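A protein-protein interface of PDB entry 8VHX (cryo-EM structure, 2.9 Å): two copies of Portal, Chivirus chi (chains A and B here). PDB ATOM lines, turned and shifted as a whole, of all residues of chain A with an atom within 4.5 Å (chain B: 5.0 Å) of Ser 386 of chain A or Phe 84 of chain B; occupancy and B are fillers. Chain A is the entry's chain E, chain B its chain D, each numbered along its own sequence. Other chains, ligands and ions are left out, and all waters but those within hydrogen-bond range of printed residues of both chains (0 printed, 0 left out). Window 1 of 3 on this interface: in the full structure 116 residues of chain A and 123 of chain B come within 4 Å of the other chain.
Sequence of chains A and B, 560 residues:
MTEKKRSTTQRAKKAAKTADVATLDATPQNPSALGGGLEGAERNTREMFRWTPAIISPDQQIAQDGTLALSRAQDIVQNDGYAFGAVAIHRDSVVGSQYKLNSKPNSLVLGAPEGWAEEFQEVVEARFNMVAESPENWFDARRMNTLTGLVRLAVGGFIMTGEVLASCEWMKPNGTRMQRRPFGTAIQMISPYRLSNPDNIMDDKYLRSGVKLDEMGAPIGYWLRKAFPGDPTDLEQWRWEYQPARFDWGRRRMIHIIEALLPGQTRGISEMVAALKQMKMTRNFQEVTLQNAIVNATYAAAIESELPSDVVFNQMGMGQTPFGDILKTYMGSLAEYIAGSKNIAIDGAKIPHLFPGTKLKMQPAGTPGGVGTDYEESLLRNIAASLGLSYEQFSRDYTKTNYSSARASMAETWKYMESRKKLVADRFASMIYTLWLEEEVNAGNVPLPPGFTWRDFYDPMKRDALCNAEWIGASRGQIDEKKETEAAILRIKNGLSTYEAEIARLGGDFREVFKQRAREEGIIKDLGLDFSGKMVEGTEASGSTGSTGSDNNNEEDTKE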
ATOM      1  N   LEU A 261     -17.223 -10.894   6.720  1.00  0.00           N
ATOM      2  CA  LEU A 261     -18.125 -10.442   7.768  1.00  0.00           C
ATOM      3  C   LEU A 261     -19.207  -9.530   7.214  1.00  0.00           C
ATOM      4  O   LEU A 261     -20.389  -9.695   7.529  1.00  0.00           O
ATOM      5  CB  LEU A 261     -17.349  -9.699   8.858  1.00  0.00           C
ATOM      6  CG  LEU A 261     -18.180  -9.218  10.055  1.00  0.00           C
ATOM      7  CD1 LEU A 261     -18.581 -10.374  10.935  1.00  0.00           C
ATOM      8  CD2 LEU A 261     -17.459  -8.164  10.877  1.00  0.00           C
ATOM      9  N   GLU A 271      -9.718 -12.729  12.286  1.00  0.00           N
ATOM     10  CA  GLU A 271     -10.469 -12.783  13.533  1.00  0.00           C
ATOM     11  C   GLU A 271      -9.722 -12.104  14.669  1.00  0.00           C
ATOM     12  O   GLU A 271     -10.348 -11.612  15.612  1.00  0.00           O
ATOM     13  CB  GLU A 271     -10.746 -14.230  13.904  1.00  0.00           C
ATOM     14  CG  GLU A 271     -11.538 -15.018  12.888  1.00  0.00           C
ATOM     15  CD  GLU A 271     -10.658 -15.799  11.941  1.00  0.00           C
ATOM     16  OE1 GLU A 271      -9.804 -15.181  11.274  1.00  0.00           O
ATOM     17  OE2 GLU A 271     -10.822 -17.035  11.867  1.00  0.00           O
ATOM     18  N   ALA A 274     -10.428  -8.300  16.188  1.00  0.00           N
ATOM     19  CA  ALA A 274     -11.393  -7.995  17.228  1.00  0.00           C
ATOM     20  C   ALA A 274     -10.765  -8.013  18.606  1.00  0.00           C
ATOM     21  O   ALA A 274     -11.324  -7.431  19.540  1.00  0.00           O
ATOM     22  CB  ALA A 274     -12.534  -8.992  17.158  1.00  0.00           C
ATOM     23  N   ALA A 275      -9.606  -8.646  18.749  1.00  0.00           N
ATOM     24  CA  ALA A 275      -9.006  -8.893  20.044  1.00  0.00           C
ATOM     25  C   ALA A 275      -7.605  -8.331  20.200  1.00  0.00           C
ATOM     26  O   ALA A 275      -7.093  -8.317  21.323  1.00  0.00           O
ATOM     27  CB  ALA A 275      -8.961 -10.398  20.312  1.00  0.00           C
ATOM     28  N   ASN A 382     -12.396 -13.584  26.689  1.00  0.00           N
ATOM     29  CA  ASN A 382     -12.732 -12.584  25.687  1.00  0.00           C
ATOM     30  C   ASN A 382     -11.935 -12.810  24.418  1.00  0.00           C
ATOM     31  O   ASN A 382     -12.460 -12.677  23.309  1.00  0.00           O
ATOM     32  CB  ASN A 382     -12.473 -11.186  26.226  1.00  0.00           C
ATOM     33  CG  ASN A 382     -12.958 -10.111  25.293  1.00  0.00           C
ATOM     34  OD1 ASN A 382     -13.150 -10.339  24.102  1.00  0.00           O
ATOM     35  ND2 ASN A 382     -13.165  -8.927  25.829  1.00  0.00           N
ATOM     36  N   ILE A 383     -10.661 -13.148  24.564  1.00  0.00           N
ATOM     37  CA  ILE A 383      -9.831 -13.379  23.388  1.00  0.00           C
ATOM     38  C   ILE A 383     -10.275 -14.636  22.650  1.00  0.00           C
ATOM     39  O   ILE A 383     -10.518 -14.617  21.436  1.00  0.00           O
ATOM     40  CB  ILE A 383      -8.354 -13.461  23.786  1.00  0.00           C
ATOM     41  CG1 ILE A 383      -7.895 -12.145  24.385  1.00  0.00           C
ATOM     42  CG2 ILE A 383      -7.540 -13.772  22.599  1.00  0.00           C
ATOM     43  CD1 ILE A 383      -6.699 -12.291  25.210  1.00  0.00           C
ATOM     44  N   ALA A 384     -10.354 -15.756  23.361  1.00  0.00           N
ATOM     45  CA  ALA A 384     -10.703 -17.015  22.726  1.00  0.00           C
ATOM     46  C   ALA A 384     -12.050 -16.934  22.032  1.00  0.00           C
ATOM     47  O   ALA A 384     -12.299 -17.651  21.058  1.00  0.00           O
ATOM     48  CB  ALA A 384     -10.698 -18.131  23.758  1.00  0.00           C
ATOM     49  N   ALA A 385     -12.938 -16.075  22.522  1.00  0.00           N
ATOM     50  CA  ALA A 385     -14.219 -15.900  21.855  1.00  0.00           C
ATOM     51  C   ALA A 385     -14.029 -15.387  20.440  1.00  0.00           C
ATOM     52  O   ALA A 385     -14.739 -15.801  19.516  1.00  0.00           O
ATOM     53  CB  ALA A 385     -15.083 -14.942  22.655  1.00  0.00           C
ATOM     54  N   SER A 386     -13.077 -14.479  20.254  1.00  0.00           N
ATOM     55  CA  SER A 386     -12.771 -13.985  18.922  1.00  0.00           C
ATOM     56  C   SER A 386     -12.015 -15.026  18.116  1.00  0.00           C
ATOM     57  O   SER A 386     -12.230 -15.158  16.908  1.00  0.00           O
ATOM     58  CB  SER A 386     -11.966 -12.698  19.022  1.00  0.00           C
ATOM     59  OG  SER A 386     -10.586 -12.969  19.110  1.00  0.00           O
ATOM     60  N   LEU A 387     -11.130 -15.773  18.763  1.00  0.00           N
ATOM     61  CA  LEU A 387     -10.382 -16.809  18.067  1.00  0.00           C
ATOM     62  C   LEU A 387     -11.189 -18.076  17.838  1.00  0.00           C
ATOM     63  O   LEU A 387     -10.686 -19.003  17.198  1.00  0.00           O
ATOM     64  CB  LEU A 387      -9.116 -17.155  18.837  1.00  0.00           C
ATOM     65  CG  LEU A 387      -8.234 -15.992  19.264  1.00  0.00           C
ATOM     66  CD1 LEU A 387      -6.960 -16.520  19.855  1.00  0.00           C
ATOM     67  CD2 LEU A 387      -7.947 -15.106  18.096  1.00  0.00           C
ATOM     68  N   GLY A 388     -12.412 -18.144  18.346  1.00  0.00           N
ATOM     69  CA  GLY A 388     -13.261 -19.295  18.141  1.00  0.00           C
ATOM     70  C   GLY A 388     -12.987 -20.459  19.054  1.00  0.00           C
ATOM     71  O   GLY A 388     -13.469 -21.563  18.786  1.00  0.00           O
ATOM     72  N   VAL B  77     -18.855  -5.027  16.926  1.00  0.00           N
ATOM     73  CA  VAL B  77     -18.499  -6.352  16.439  1.00  0.00           C
ATOM     74  C   VAL B  77     -17.027  -6.410  16.064  1.00  0.00           C
ATOM     75  O   VAL B  77     -16.345  -7.409  16.320  1.00  0.00           O
ATOM     76  CB  VAL B  77     -19.392  -6.738  15.255  1.00  0.00           C
ATOM     77  CG1 VAL B  77     -18.827  -7.897  14.539  1.00  0.00           C
ATOM     78  CG2 VAL B  77     -20.746  -7.089  15.736  1.00  0.00           C
ATOM     79  N   ASP B  80     -14.746  -5.836  19.660  1.00  0.00           N
ATOM     80  CA  ASP B  80     -14.951  -6.629  20.861  1.00  0.00           C
ATOM     81  C   ASP B  80     -14.968  -8.096  20.461  1.00  0.00           C
ATOM     82  O   ASP B  80     -15.644  -8.471  19.497  1.00  0.00           O
ATOM     83  CB  ASP B  80     -16.252  -6.236  21.559  1.00  0.00           C
ATOM     84  CG  ASP B  80     -16.312  -6.697  23.001  1.00  0.00           C
ATOM     85  OD1 ASP B  80     -17.431  -6.944  23.502  1.00  0.00           O
ATOM     86  OD2 ASP B  80     -15.245  -6.799  23.642  1.00  0.00           O
ATOM     87  N   GLY B  81     -14.205  -8.915  21.185  1.00  0.00           N
ATOM     88  CA  GLY B  81     -14.155 -10.335  20.891  1.00  0.00           C
ATOM     89  C   GLY B  81     -15.439 -11.061  21.211  1.00  0.00           C
ATOM     90  O   GLY B  81     -15.768 -12.060  20.570  1.00  0.00           O
ATOM     91  N   TYR B  82     -16.188 -10.569  22.190  1.00  0.00           N
ATOM     92  CA  TYR B  82     -17.416 -11.243  22.581  1.00  0.00           C
ATOM     93  C   TYR B  82     -18.495 -11.100  21.519  1.00  0.00           C
ATOM     94  O   TYR B  82     -19.176 -12.073  21.183  1.00  0.00           O
ATOM     95  CB  TYR B  82     -17.904 -10.692  23.915  1.00  0.00           C
ATOM     96  CG  TYR B  82     -17.214 -11.249  25.135  1.00  0.00           C
ATOM     97  CD1 TYR B  82     -16.979 -12.601  25.263  1.00  0.00           C
ATOM     98  CD2 TYR B  82     -16.839 -10.427  26.180  1.00  0.00           C
ATOM     99  CE1 TYR B  82     -16.371 -13.105  26.360  1.00  0.00           C
ATOM    100  CE2 TYR B  82     -16.230 -10.935  27.292  1.00  0.00           C
ATOM    101  CZ  TYR B  82     -16.003 -12.277  27.380  1.00  0.00           C
ATOM    102  OH  TYR B  82     -15.393 -12.805  28.491  1.00  0.00           O
ATOM    103  N   ALA B  83     -18.659  -9.901  20.969  1.00  0.00           N
ATOM    104  CA  ALA B  83     -19.639  -9.703  19.911  1.00  0.00           C
ATOM    105  C   ALA B  83     -19.243 -10.432  18.632  1.00  0.00           C
ATOM    106  O   ALA B  83     -20.093 -11.023  17.956  1.00  0.00           O
ATOM    107  CB  ALA B  83     -19.809  -8.216  19.657  1.00  0.00           C
ATOM    108  N   PHE B  84     -17.965 -10.379  18.270  1.00  0.00           N
ATOM    109  CA  PHE B  84     -17.489 -11.143  17.125  1.00  0.00           C
ATOM    110  C   PHE B  84     -17.767 -12.628  17.309  1.00  0.00           C
ATOM    111  O   PHE B  84     -18.239 -13.308  16.384  1.00  0.00           O
ATOM    112  CB  PHE B  84     -16.000 -10.875  16.944  1.00  0.00           C
ATOM    113  CG  PHE B  84     -15.449 -11.347  15.644  1.00  0.00           C
ATOM    114  CD1 PHE B  84     -15.562 -10.568  14.519  1.00  0.00           C
ATOM    115  CD2 PHE B  84     -14.791 -12.552  15.551  1.00  0.00           C
ATOM    116  CE1 PHE B  84     -15.053 -10.990  13.332  1.00  0.00           C
ATOM    117  CE2 PHE B  84     -14.284 -12.973  14.363  1.00  0.00           C
ATOM    118  CZ  PHE B  84     -14.414 -12.193  13.253  1.00  0.00           C
ATOM    119  N   GLY B  85     -17.498 -13.147  18.505  1.00  0.00           N
ATOM    120  CA  GLY B  85     -17.828 -14.529  18.789  1.00  0.00           C
ATOM    121  C   GLY B  85     -19.312 -14.803  18.694  1.00  0.00           C
ATOM    122  O   GLY B  85     -19.725 -15.881  18.274  1.00  0.00           O
ATOM    123  N   ALA B  86     -20.135 -13.840  19.108  1.00  0.00           N
ATOM    124  CA  ALA B  86     -21.579 -13.999  18.989  1.00  0.00           C
ATOM    125  C   ALA B  86     -21.998 -14.124  17.537  1.00  0.00           C
ATOM    126  O   ALA B  86     -22.851 -14.950  17.192  1.00  0.00           O
ATOM    127  CB  ALA B  86     -22.286 -12.817  19.636  1.00  0.00           C
ATOM    128  N   VAL B  87     -21.421 -13.295  16.674  1.00  0.00           N
ATOM    129  CA  VAL B  87     -21.720 -13.387  15.250  1.00  0.00           C
ATOM    130  C   VAL B  87     -21.331 -14.759  14.728  1.00  0.00           C
ATOM    131  O   VAL B  87     -22.084 -15.401  13.983  1.00  0.00           O
ATOM    132  CB  VAL B  87     -21.001 -12.271  14.475  1.00  0.00           C
ATOM    133  CG1 VAL B  87     -21.273 -12.413  13.018  1.00  0.00           C
ATOM    134  CG2 VAL B  87     -21.441 -10.915  14.940  1.00  0.00           C
ATOM    135  N   ALA B  88     -20.143 -15.225  15.107  1.00  0.00           N
ATOM    136  CA  ALA B  88     -19.708 -16.547  14.680  1.00  0.00           C
ATOM    137  C   ALA B  88     -20.650 -17.626  15.188  1.00  0.00           C
ATOM    138  O   ALA B  88     -20.944 -18.590  14.476  1.00  0.00           O
ATOM    139  CB  ALA B  88     -18.293 -16.806  15.165  1.00  0.00           C
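No position is printed for both chains.
Of the 14 pairs that touch across the chains among the printed residues, none has its exchanged pair printed and touching as well.
The side-chain hydroxyl (OG) of Ser 386 of chain A lies within hydrogen-bond range of the backbone carbonyl oxygen (O) of Ile 383 of chain A.
Of the printed residues of chain B, Ala 274 of chain A touches Asp 80, Gly 81 and Phe 84.
Of the printed residues of chain A, Gly 81 of chain B touches Ala 274, Asn 382, Ala 385 and Ser 386.
Of the printed residues of chain A, Tyr 82 of chain B touches Asn 382 (3.6 Å) and Ala 385 (3.98 Å).
Phe 84 of chain B touches just these residues of chain A: Glu 271, Ala 274 and Ser 386.
Printed residues of chain A within 4 Å of Gly 85 of chain B: Ala 385 (3.4 Å).
The nearest residue of chain A that does not touch Phe 84 of chain B is Leu 261 of chain A (4.3 Å).
Among the printed residues, pairs that only touch across the chains: Leu 261 of chain A with Val 77 of chain B, Leu 261 of chain A with Val 87 of chain B, Glu 271 of chain A with Phe 84 of chain B, Ala 274 of chain A with Asp 80 of chain B, Ala 274 of chain A with Gly 81 of chain B, Ala 274 of chain A with Phe 84 of chain B, Asn 382 of chain A with Asp 80 of chain B, Asn 382 of chain A with Tyr 82 of chain B, Ala 385 of chain A with Gly 81 of chain B, Ala 385 of chain A with Tyr 82 of chain B, Ala 385 of chain A with Gly 85 of chain B, Ser 386 of chain A with Gly 81 of chain B and Ser 386 of chain A with Phe 84 of chain B.
N of Gly 81 of chain B lies close to OD1 of Asn 382 of chain A (3.4 Å).
Hydrophobic or aromatic side chains of chain B within 4 Å of the printed part of chain A: Val 77, Tyr 82, Phe 84 and Val 87.
Of the 11 printed residues of chain A, 6 touch a printed residue of chain B.
Hydrophobic or aromatic side chains of chain A that line the printed part of chain B: Leu 261, Ala 274 and Ala 385.
Among the printed residues, 14 pairs touch across the chains.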
